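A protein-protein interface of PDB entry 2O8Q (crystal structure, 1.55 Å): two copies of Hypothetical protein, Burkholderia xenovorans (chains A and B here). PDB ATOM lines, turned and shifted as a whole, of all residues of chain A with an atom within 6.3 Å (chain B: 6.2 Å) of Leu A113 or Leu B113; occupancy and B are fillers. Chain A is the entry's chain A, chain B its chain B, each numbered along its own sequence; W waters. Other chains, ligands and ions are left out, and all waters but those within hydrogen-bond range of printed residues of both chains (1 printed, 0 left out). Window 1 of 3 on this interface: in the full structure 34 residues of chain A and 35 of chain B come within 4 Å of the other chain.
Printed residues of chain B within 4 Å of Leu A71: Tyr B69 and Leu B71.
Of chain B, only Tyr B69 (3.8 Å) and Leu B113 (3.8 Å) come within 4 Å of Leu A113.
Printed residues of chain A within 4 Å of Ala B43: Leu A67 (3.5 Å).
Printed residues of chain A within 4 Å of Leu B67: Ala A43.
Of the printed residues of chain A, Leu B71 touches Tyr A69 and Leu A71.
Printed residues of chain A within 4 Å of Leu B113: Tyr A69 (3.8 Å) and Leu A113 (3.8 Å).
The nearest residue of chain B that does not touch Leu A113 is Ile B115 (4.7 Å).
Among the printed residues, merely in contact across the chains: Leu A71 with Leu B71 (3.4 Å), Tyr A69 with Val B45 (3.5 Å), Ala A43 with Leu B67 (3.5 Å), Val A45 with Tyr B69 (3.5 Å), Leu A67 with Ala B43 (3.5 Å), Tyr A69 with Leu B71 (3.6 Å), Leu A71 with Tyr B69 (3.6 Å), Leu A113 with Tyr B69 (3.8 Å), Leu A113 with Leu B113 (3.8 Å) and Tyr A69 with Leu B113 (3.8 Å).
OG1 of Thr A31 is in hydrogen-bond range of O of Ala A43 (2.6 Å).
The backbone NH (N) of Leu A67 lies within hydrogen-bond range of the backbone carbonyl oxygen (O) of Ile A115 (2.9 Å).
The backbone NH of Tyr A69 lies within hydrogen-bond range of the backbone carbonyl oxygen of Leu A113.
O of Ala B43 sits at hydrogen-bond distance from OG1 of Thr B31 (2.7 Å).
The backbone NH (N) of Ile B115 is in hydrogen-bond range of the backbone carbonyl oxygen (O) of Leu B67.
The backbone NH (N) of Leu B113 is in hydrogen-bond range of the backbone carbonyl oxygen (O) of Tyr B69.
Water W1 lies within hydrogen-bond range of OH of Tyr A69 and OE2 of Glu B111.
Hydrophobic or aromatic side chains of chain B that line the printed part of chain A: Ala B43, Val B45, Leu B67, Tyr B69, Leu B71 and Leu B113.
Of the 15 printed residues of chain A, 6 touch a printed residue of chain B.
Hydrophobic or aromatic side chains of chain A that line the printed part of chain B: Ala A43, Val A45, Leu A67, Tyr A69, Leu A71 and Leu A113.
Among the printed residues, 10 pairs touch across the chains.
Among the printed residues, no Asp or Glu carboxylate lies within 4 Å of a Lys or Arg side-chain nitrogen of the other chain.
Tyr A69 touches Leu B71, and with the chains exchanged Leu A71 touches Tyr B69.
Tyr A69 touches Leu B113, and with the chains exchanged Leu A113 touches Tyr B69.
Leu B71 touches its own counterpart, Leu A71.
Leu B113 touches its own counterpart, Leu A113.
Positions printed for both chains: 31, 43, 44, 45, 46, 67, 68, 69, 70, 71, 111, 112, 113, 114 and 115.
Of the 10 pairs that touch across the chains among the printed residues, 10 have their exchanged pair printed and touching as well.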
ATOM      1  N   THR A  31      29.179 -11.536   5.766  1.00  0.00           N
ATOM      2  CA  THR A  31      28.962 -12.863   6.373  1.00  0.00           C
ATOM      3  C   THR A  31      30.057 -13.246   7.386  1.00  0.00           C
ATOM      4  O   THR A  31      29.913 -14.201   8.182  1.00  0.00           O
ATOM      5  CB  THR A  31      29.035 -13.958   5.321  1.00  0.00           C
ATOM      6  OG1 THR A  31      30.336 -13.975   4.684  1.00  0.00           O
ATOM      7  CG2 THR A  31      27.901 -13.810   4.299  1.00  0.00           C
ATOM      8  N   ALA A  43      32.456 -13.095   1.458  1.00  0.00           N
ATOM      9  CA  ALA A  43      31.086 -13.233   1.011  1.00  0.00           C
ATOM     10  C   ALA A  43      30.273 -12.198   1.729  1.00  0.00           C
ATOM     11  O   ALA A  43      30.419 -11.978   2.945  1.00  0.00           O
ATOM     12  CB  ALA A  43      30.535 -14.625   1.287  1.00  0.00           C
ATOM     13  N   HIS A  44      29.422 -11.548   0.982  1.00  0.00           N
ATOM     14  CA  HIS A  44      28.620 -10.434   1.526  1.00  0.00           C
ATOM     15  C   HIS A  44      27.369 -10.255   0.732  1.00  0.00           C
ATOM     16  O   HIS A  44      27.295 -10.616  -0.430  1.00  0.00           O
ATOM     17  CB  HIS A  44      29.465  -9.170   1.593  1.00  0.00           C
ATOM     18  CG  HIS A  44      30.245  -8.966   0.333  1.00  0.00           C
ATOM     19  ND1 HIS A  44      31.585  -9.312   0.230  1.00  0.00           N
ATOM     20  CD2 HIS A  44      29.834  -8.659  -0.915  1.00  0.00           C
ATOM     21  CE1 HIS A  44      31.976  -9.116  -1.019  1.00  0.00           C
ATOM     22  NE2 HIS A  44      30.947  -8.647  -1.717  1.00  0.00           N
ATOM     23  N   VAL A  45      26.355  -9.682   1.378  1.00  0.00           N
ATOM     24  CA  VAL A  45      25.104  -9.338   0.709  1.00  0.00           C
ATOM     25  C   VAL A  45      25.154  -7.845   0.333  1.00  0.00           C
ATOM     26  O   VAL A  45      25.528  -6.963   1.144  1.00  0.00           O
ATOM     27  CB  VAL A  45      23.888  -9.648   1.565  1.00  0.00           C
ATOM     28  CG1 VAL A  45      22.558  -9.192   0.884  1.00  0.00           C
ATOM     29  CG2 VAL A  45      23.859 -11.152   1.953  1.00  0.00           C
ATOM     30  N   ILE A  46      24.811  -7.592  -0.913  1.00  0.00           N
ATOM     31  CA  ILE A  46      24.843  -6.263  -1.474  1.00  0.00           C
ATOM     32  C   ILE A  46      23.396  -5.831  -1.700  1.00  0.00           C
ATOM     33  O   ILE A  46      22.613  -6.562  -2.272  1.00  0.00           O
ATOM     34  CB  ILE A  46      25.560  -6.279  -2.827  1.00  0.00           C
ATOM     35  CG1 ILE A  46      26.929  -6.985  -2.742  1.00  0.00           C
ATOM     36  CG2 ILE A  46      25.727  -4.843  -3.395  1.00  0.00           C
ATOM     37  CD1 ILE A  46      27.698  -7.030  -4.012  1.00  0.00           C
ATOM     38  N   LEU A  67      31.016 -15.485  -7.674  1.00  0.00           N
ATOM     39  CA  LEU A  67      29.633 -15.898  -7.927  1.00  0.00           C
ATOM     40  C   LEU A  67      28.649 -14.939  -7.319  1.00  0.00           C
ATOM     41  O   LEU A  67      28.845 -14.512  -6.177  1.00  0.00           O
ATOM     42  CB  LEU A  67      29.370 -17.274  -7.268  1.00  0.00           C
ATOM     43  CG  LEU A  67      27.998 -17.935  -7.449  1.00  0.00           C
ATOM     44  CD1 LEU A  67      27.624 -18.243  -8.910  1.00  0.00           C
ATOM     45  CD2 LEU A  67      27.921 -19.238  -6.613  1.00  0.00           C
ATOM     46  N   PHE A  68      27.584 -14.595  -8.057  1.00  0.00           N
ATOM     47  CA  PHE A  68      26.475 -13.803  -7.534  1.00  0.00           C
ATOM     48  C   PHE A  68      25.222 -14.665  -7.528  1.00  0.00           C
ATOM     49  O   PHE A  68      24.969 -15.432  -8.487  1.00  0.00           O
ATOM     50  CB  PHE A  68      26.193 -12.607  -8.448  1.00  0.00           C
ATOM     51  CG  PHE A  68      27.313 -11.612  -8.422  1.00  0.00           C
ATOM     52  CD1 PHE A  68      27.410 -10.667  -7.406  1.00  0.00           C
ATOM     53  CD2 PHE A  68      28.360 -11.723  -9.300  1.00  0.00           C
ATOM     54  CE1 PHE A  68      28.486  -9.808  -7.344  1.00  0.00           C
ATOM     55  CE2 PHE A  68      29.419 -10.859  -9.216  1.00  0.00           C
ATOM     56  CZ  PHE A  68      29.497  -9.925  -8.247  1.00  0.00           C
ATOM     57  N   TYR A  69      24.460 -14.526  -6.448  1.00  0.00           N
ATOM     58  CA  TYR A  69      23.133 -15.172  -6.315  1.00  0.00           C
ATOM     59  C   TYR A  69      22.135 -14.105  -5.901  1.00  0.00           C
ATOM     60  O   TYR A  69      22.244 -13.531  -4.869  1.00  0.00           O
ATOM     61  CB  TYR A  69      23.160 -16.334  -5.314  1.00  0.00           C
ATOM     62  CG  TYR A  69      21.897 -17.168  -5.311  1.00  0.00           C
ATOM     63  CD1 TYR A  69      20.803 -16.745  -4.580  1.00  0.00           C
ATOM     64  CD2 TYR A  69      21.781 -18.307  -6.088  1.00  0.00           C
ATOM     65  CE1 TYR A  69      19.634 -17.487  -4.599  1.00  0.00           C
ATOM     66  CE2 TYR A  69      20.638 -19.049  -6.095  1.00  0.00           C
ATOM     67  CZ  TYR A  69      19.556 -18.640  -5.363  1.00  0.00           C
ATOM     68  OH  TYR A  69      18.378 -19.381  -5.384  1.00  0.00           O
ATOM     69  N   VAL A  70      21.153 -13.846  -6.751  1.00  0.00           N
ATOM     70  CA  VAL A  70      20.176 -12.790  -6.485  1.00  0.00           C
ATOM     71  C   VAL A  70      19.128 -13.243  -5.480  1.00  0.00           C
ATOM     72  O   VAL A  70      18.449 -14.257  -5.657  1.00  0.00           O
ATOM     73  CB  VAL A  70      19.515 -12.281  -7.773  1.00  0.00           C
ATOM     74  CG1 VAL A  70      18.515 -11.161  -7.417  1.00  0.00           C
ATOM     75  CG2 VAL A  70      20.584 -11.793  -8.744  1.00  0.00           C
ATOM     76  N   LEU A  71      18.992 -12.451  -4.401  1.00  0.00           N
ATOM     77  CA  LEU A  71      18.074 -12.781  -3.294  1.00  0.00           C
ATOM     78  C   LEU A  71      16.721 -12.067  -3.435  1.00  0.00           C
ATOM     79  O   LEU A  71      15.698 -12.540  -2.942  1.00  0.00           O
ATOM     80  CB  LEU A  71      18.747 -12.404  -1.966  1.00  0.00           C
ATOM     81  CG  LEU A  71      20.069 -13.122  -1.670  1.00  0.00           C
ATOM     82  CD1 LEU A  71      20.773 -12.465  -0.472  1.00  0.00           C
ATOM     83  CD2 LEU A  71      19.832 -14.625  -1.461  1.00  0.00           C
ATOM     84  N   GLU A 111      18.823  -7.185  -3.869  1.00  0.00           N
ATOM     85  CA  GLU A 111      19.705  -7.768  -2.843  1.00  0.00           C
ATOM     86  C   GLU A 111      20.387  -8.975  -3.463  1.00  0.00           C
ATOM     87  O   GLU A 111      19.696  -9.847  -3.977  1.00  0.00           O
ATOM     88  CB  GLU A 111      18.870  -8.195  -1.638  1.00  0.00           C
ATOM     89  CG  GLU A 111      19.691  -8.539  -0.398  1.00  0.00           C
ATOM     90  CD  GLU A 111      18.826  -8.867   0.810  1.00  0.00           C
ATOM     91  OE1 GLU A 111      17.657  -9.268   0.612  1.00  0.00           O
ATOM     92  OE2 GLU A 111      19.315  -8.733   1.947  1.00  0.00           O
ATOM     93  N   VAL A 112      21.718  -9.036  -3.412  1.00  0.00           N
ATOM     94  CA  VAL A 112      22.467 -10.071  -4.091  1.00  0.00           C
ATOM     95  C   VAL A 112      23.598 -10.522  -3.188  1.00  0.00           C
ATOM     96  O   VAL A 112      24.317  -9.691  -2.625  1.00  0.00           O
ATOM     97  CB  VAL A 112      22.939  -9.579  -5.504  1.00  0.00           C
ATOM     98  CG1 VAL A 112      23.800  -8.348  -5.409  1.00  0.00           C
ATOM     99  CG2 VAL A 112      23.631 -10.720  -6.279  1.00  0.00           C
ATOM    100  N   LEU A 113      23.802 -11.820  -3.099  1.00  0.00           N
ATOM    101  CA  LEU A 113      24.936 -12.380  -2.383  1.00  0.00           C
ATOM    102  C   LEU A 113      26.091 -12.553  -3.375  1.00  0.00           C
ATOM    103  O   LEU A 113      25.933 -13.088  -4.462  1.00  0.00           O
ATOM    104  CB  LEU A 113      24.546 -13.747  -1.824  1.00  0.00           C
ATOM    105  CG  LEU A 113      25.609 -14.548  -1.070  1.00  0.00           C
ATOM    106  CD1 LEU A 113      26.044 -13.874   0.257  1.00  0.00           C
ATOM    107  CD2 LEU A 113      25.112 -16.036  -0.833  1.00  0.00           C
ATOM    108  N   GLU A 114      27.262 -12.091  -2.964  1.00  0.00           N
ATOM    109  CA  GLU A 114      28.489 -12.226  -3.721  1.00  0.00           C
ATOM    110  C   GLU A 114      29.432 -13.093  -2.887  1.00  0.00           C
ATOM    111  O   GLU A 114      29.622 -12.820  -1.713  1.00  0.00           O
ATOM    112  CB  GLU A 114      29.191 -10.879  -3.989  1.00  0.00           C
ATOM    113  CG  GLU A 114      30.505 -10.995  -4.784  1.00  0.00           C
ATOM    114  CD  GLU A 114      31.126  -9.670  -5.133  1.00  0.00           C
ATOM    115  OE1 GLU A 114      30.824  -8.640  -4.459  1.00  0.00           O
ATOM    116  OE2 GLU A 114      31.962  -9.611  -6.080  1.00  0.00           O
ATOM    117  N   ILE A 115      30.021 -14.107  -3.540  1.00  0.00           N
ATOM    118  CA  ILE A 115      31.053 -14.970  -2.970  1.00  0.00           C
ATOM    119  C   ILE A 115      32.266 -14.821  -3.876  1.00  0.00           C
ATOM    120  O   ILE A 115      32.160 -15.002  -5.076  1.00  0.00           O
ATOM    121  CB  ILE A 115      30.623 -16.438  -2.879  1.00  0.00           C
ATOM    122  CG1 ILE A 115      29.220 -16.567  -2.279  1.00  0.00           C
ATOM    123  CG2 ILE A 115      31.724 -17.248  -2.148  1.00  0.00           C
ATOM    124  CD1 ILE A 115      28.056 -16.665  -3.302  1.00  0.00           C
ATOM    125  N   THR B  31      23.645 -24.461 -10.029  1.00  0.00           N
ATOM    126  CA  THR B  31      23.936 -23.166 -10.658  1.00  0.00           C
ATOM    127  C   THR B  31      24.765 -23.292 -11.920  1.00  0.00           C
ATOM    128  O   THR B  31      24.909 -22.316 -12.693  1.00  0.00           O
ATOM    129  CB  THR B  31      24.769 -22.267  -9.726  1.00  0.00           C
ATOM    130  OG1 THR B  31      26.010 -22.939  -9.439  1.00  0.00           O
ATOM    131  CG2 THR B  31      23.982 -21.935  -8.410  1.00  0.00           C
ATOM    132  N   ALA B  43      28.169 -25.009  -6.719  1.00  0.00           N
ATOM    133  CA  ALA B  43      27.198 -24.194  -6.022  1.00  0.00           C
ATOM    134  C   ALA B  43      25.818 -24.644  -6.428  1.00  0.00           C
ATOM    135  O   ALA B  43      25.521 -24.819  -7.589  1.00  0.00           O
ATOM    136  CB  ALA B  43      27.388 -22.728  -6.260  1.00  0.00           C
ATOM    137  N   HIS B  44      24.980 -24.859  -5.440  1.00  0.00           N
ATOM    138  CA  HIS B  44      23.659 -25.420  -5.711  1.00  0.00           C
ATOM    139  C   HIS B  44      22.713 -25.050  -4.578  1.00  0.00           C
ATOM    140  O   HIS B  44      23.127 -24.761  -3.440  1.00  0.00           O
ATOM    141  CB  HIS B  44      23.749 -26.916  -5.880  1.00  0.00           C
ATOM    142  CG  HIS B  44      24.643 -27.537  -4.866  1.00  0.00           C
ATOM    143  ND1 HIS B  44      25.942 -27.918  -5.165  1.00  0.00           N
ATOM    144  CD2 HIS B  44      24.499 -27.679  -3.534  1.00  0.00           C
ATOM    145  CE1 HIS B  44      26.528 -28.334  -4.057  1.00  0.00           C
ATOM    146  NE2 HIS B  44      25.660 -28.246  -3.058  1.00  0.00           N
ATOM    147  N   VAL B  45      21.437 -25.003  -4.913  1.00  0.00           N
ATOM    148  CA  VAL B  45      20.401 -24.763  -3.915  1.00  0.00           C
ATOM    149  C   VAL B  45      19.806 -26.109  -3.475  1.00  0.00           C
ATOM    150  O   VAL B  45      19.551 -26.978  -4.295  1.00  0.00           O
ATOM    151  CB  VAL B  45      19.260 -23.852  -4.476  1.00  0.00           C
ATOM    152  CG1 VAL B  45      18.155 -23.703  -3.429  1.00  0.00           C
ATOM    153  CG2 VAL B  45      19.868 -22.488  -4.856  1.00  0.00           C
ATOM    154  N   ILE B  46      19.749 -26.289  -2.179  1.00  0.00           N
ATOM    155  CA  ILE B  46      19.287 -27.518  -1.573  1.00  0.00           C
ATOM    156  C   ILE B  46      17.916 -27.249  -0.972  1.00  0.00           C
ATOM    157  O   ILE B  46      17.755 -26.300  -0.202  1.00  0.00           O
ATOM    158  CB  ILE B  46      20.258 -27.978  -0.451  1.00  0.00           C
ATOM    159  CG1 ILE B  46      21.724 -27.976  -0.955  1.00  0.00           C
ATOM    160  CG2 ILE B  46      19.828 -29.375   0.089  1.00  0.00           C
ATOM    161  CD1 ILE B  46      22.753 -28.317   0.099  1.00  0.00           C
ATOM    162  N   LEU B  67      30.431 -22.799   2.316  1.00  0.00           N
ATOM    163  CA  LEU B  67      29.553 -21.796   2.864  1.00  0.00           C
ATOM    164  C   LEU B  67      28.104 -22.116   2.591  1.00  0.00           C
ATOM    165  O   LEU B  67      27.774 -22.516   1.477  1.00  0.00           O
ATOM    166  CB  LEU B  67      29.889 -20.449   2.231  1.00  0.00           C
ATOM    167  CG  LEU B  67      29.077 -19.238   2.652  1.00  0.00           C
ATOM    168  CD1 LEU B  67      29.208 -18.866   4.151  1.00  0.00           C
ATOM    169  CD2 LEU B  67      29.444 -17.960   1.779  1.00  0.00           C
ATOM    170  N   PHE B  68      27.229 -21.893   3.584  1.00  0.00           N
ATOM    171  CA  PHE B  68      25.782 -22.022   3.405  1.00  0.00           C
ATOM    172  C   PHE B  68      25.158 -20.674   3.679  1.00  0.00           C
ATOM    173  O   PHE B  68      25.534 -19.972   4.594  1.00  0.00           O
ATOM    174  CB  PHE B  68      25.239 -23.003   4.431  1.00  0.00           C
ATOM    175  CG  PHE B  68      25.663 -24.411   4.145  1.00  0.00           C
ATOM    176  CD1 PHE B  68      24.967 -25.209   3.271  1.00  0.00           C
ATOM    177  CD2 PHE B  68      26.804 -24.896   4.705  1.00  0.00           C
ATOM    178  CE1 PHE B  68      25.394 -26.492   3.004  1.00  0.00           C
ATOM    179  CE2 PHE B  68      27.239 -26.174   4.431  1.00  0.00           C
ATOM    180  CZ  PHE B  68      26.531 -26.969   3.605  1.00  0.00           C
ATOM    181  N   TYR B  69      24.133 -20.395   2.888  1.00  0.00           N
ATOM    182  CA  TYR B  69      23.302 -19.194   3.049  1.00  0.00           C
ATOM    183  C   TYR B  69      21.837 -19.640   2.945  1.00  0.00           C
ATOM    184  O   TYR B  69      21.398 -20.167   1.900  1.00  0.00           O
ATOM    185  CB  TYR B  69      23.609 -18.148   1.957  1.00  0.00           C
ATOM    186  CG  TYR B  69      22.996 -16.821   2.207  1.00  0.00           C
ATOM    187  CD1 TYR B  69      21.663 -16.578   1.859  1.00  0.00           C
ATOM    188  CD2 TYR B  69      23.672 -15.820   2.871  1.00  0.00           C
ATOM    189  CE1 TYR B  69      21.060 -15.367   2.127  1.00  0.00           C
ATOM    190  CE2 TYR B  69      23.050 -14.581   3.166  1.00  0.00           C
ATOM    191  CZ  TYR B  69      21.743 -14.353   2.779  1.00  0.00           C
ATOM    192  OH  TYR B  69      21.147 -13.145   3.074  1.00  0.00           O
ATOM    193  N   VAL B  70      21.088 -19.384   4.005  1.00  0.00           N
ATOM    194  CA  VAL B  70      19.701 -19.864   4.090  1.00  0.00           C
ATOM    195  C   VAL B  70      18.796 -18.889   3.334  1.00  0.00           C
ATOM    196  O   VAL B  70      18.796 -17.673   3.581  1.00  0.00           O
ATOM    197  CB  VAL B  70      19.212 -20.064   5.525  1.00  0.00           C
ATOM    198  CG1 VAL B  70      17.726 -20.519   5.587  1.00  0.00           C
ATOM    199  CG2 VAL B  70      20.141 -21.084   6.209  1.00  0.00           C
ATOM    200  N   LEU B  71      18.028 -19.478   2.413  1.00  0.00           N
ATOM    201  CA  LEU B  71      17.138 -18.723   1.548  1.00  0.00           C
ATOM    202  C   LEU B  71      15.671 -18.707   2.039  1.00  0.00           C
ATOM    203  O   LEU B  71      14.913 -17.736   1.832  1.00  0.00           O
ATOM    204  CB  LEU B  71      17.197 -19.328   0.137  1.00  0.00           C
ATOM    205  CG  LEU B  71      18.538 -19.325  -0.608  1.00  0.00           C
ATOM    206  CD1 LEU B  71      18.551 -20.134  -1.866  1.00  0.00           C
ATOM    207  CD2 LEU B  71      19.072 -17.903  -0.858  1.00  0.00           C
ATOM    208  N   GLU B 111      15.270 -24.026   2.211  1.00  0.00           N
ATOM    209  CA  GLU B 111      16.026 -23.839   0.978  1.00  0.00           C
ATOM    210  C   GLU B 111      17.326 -23.148   1.378  1.00  0.00           C
ATOM    211  O   GLU B 111      17.299 -22.107   2.046  1.00  0.00           O
ATOM    212  CB  GLU B 111      15.240 -22.997  -0.055  1.00  0.00           C
ATOM    213  CG  GLU B 111      15.885 -22.932  -1.451  1.00  0.00           C
ATOM    214  CD  GLU B 111      14.956 -22.378  -2.549  1.00  0.00           C
ATOM    215  OE1 GLU B 111      13.795 -22.824  -2.590  1.00  0.00           O
ATOM    216  OE2 GLU B 111      15.413 -21.525  -3.372  1.00  0.00           O
ATOM    217  N   VAL B 112      18.454 -23.729   0.993  1.00  0.00           N
ATOM    218  CA  VAL B 112      19.752 -23.176   1.367  1.00  0.00           C
ATOM    219  C   VAL B 112      20.719 -23.299   0.184  1.00  0.00           C
ATOM    220  O   VAL B 112      20.796 -24.331  -0.491  1.00  0.00           O
ATOM    221  CB  VAL B 112      20.301 -23.880   2.648  1.00  0.00           C
ATOM    222  CG1 VAL B 112      20.428 -25.366   2.465  1.00  0.00           C
ATOM    223  CG2 VAL B 112      21.624 -23.305   3.120  1.00  0.00           C
ATOM    224  N   LEU B 113      21.456 -22.230  -0.068  1.00  0.00           N
ATOM    225  CA  LEU B 113      22.495 -22.227  -1.059  1.00  0.00           C
ATOM    226  C   LEU B 113      23.823 -22.733  -0.424  1.00  0.00           C
ATOM    227  O   LEU B 113      24.225 -22.237   0.640  1.00  0.00           O
ATOM    228  CB  LEU B 113      22.716 -20.812  -1.538  1.00  0.00           C
ATOM    229  CG  LEU B 113      23.784 -20.623  -2.617  1.00  0.00           C
ATOM    230  CD1 LEU B 113      23.512 -21.349  -3.917  1.00  0.00           C
ATOM    231  CD2 LEU B 113      24.064 -19.100  -2.830  1.00  0.00           C
ATOM    232  N   GLU B 114      24.480 -23.698  -1.086  1.00  0.00           N
ATOM    233  CA  GLU B 114      25.770 -24.190  -0.683  1.00  0.00           C
ATOM    234  C   GLU B 114      26.798 -23.823  -1.746  1.00  0.00           C
ATOM    235  O   GLU B 114      26.531 -24.082  -2.925  1.00  0.00           O
ATOM    236  CB  GLU B 114      25.768 -25.719  -0.547  1.00  0.00           C
ATOM    237  CG  GLU B 114      27.146 -26.299  -0.123  1.00  0.00           C
ATOM    238  CD  GLU B 114      27.100 -27.804   0.154  1.00  0.00           C
ATOM    239  OE1 GLU B 114      26.270 -28.546  -0.446  1.00  0.00           O
ATOM    240  OE2 GLU B 114      27.992 -28.274   0.882  1.00  0.00           O
ATOM    241  N   ILE B 115      27.928 -23.243  -1.345  1.00  0.00           N
ATOM    242  CA  ILE B 115      29.040 -22.950  -2.234  1.00  0.00           C
ATOM    243  C   ILE B 115      30.212 -23.740  -1.670  1.00  0.00           C
ATOM    244  O   ILE B 115      30.492 -23.630  -0.481  1.00  0.00           O
ATOM    245  CB  ILE B 115      29.374 -21.462  -2.264  1.00  0.00           C
ATOM    246  CG1 ILE B 115      28.091 -20.633  -2.493  1.00  0.00           C
ATOM    247  CG2 ILE B 115      30.406 -21.233  -3.408  1.00  0.00           C
ATOM    248  CD1 ILE B 115      27.417 -20.057  -1.224  1.00  0.00           C
HETATM  249  O   HOH W   1      16.213 -18.285  -4.199  1.00  0.00           O
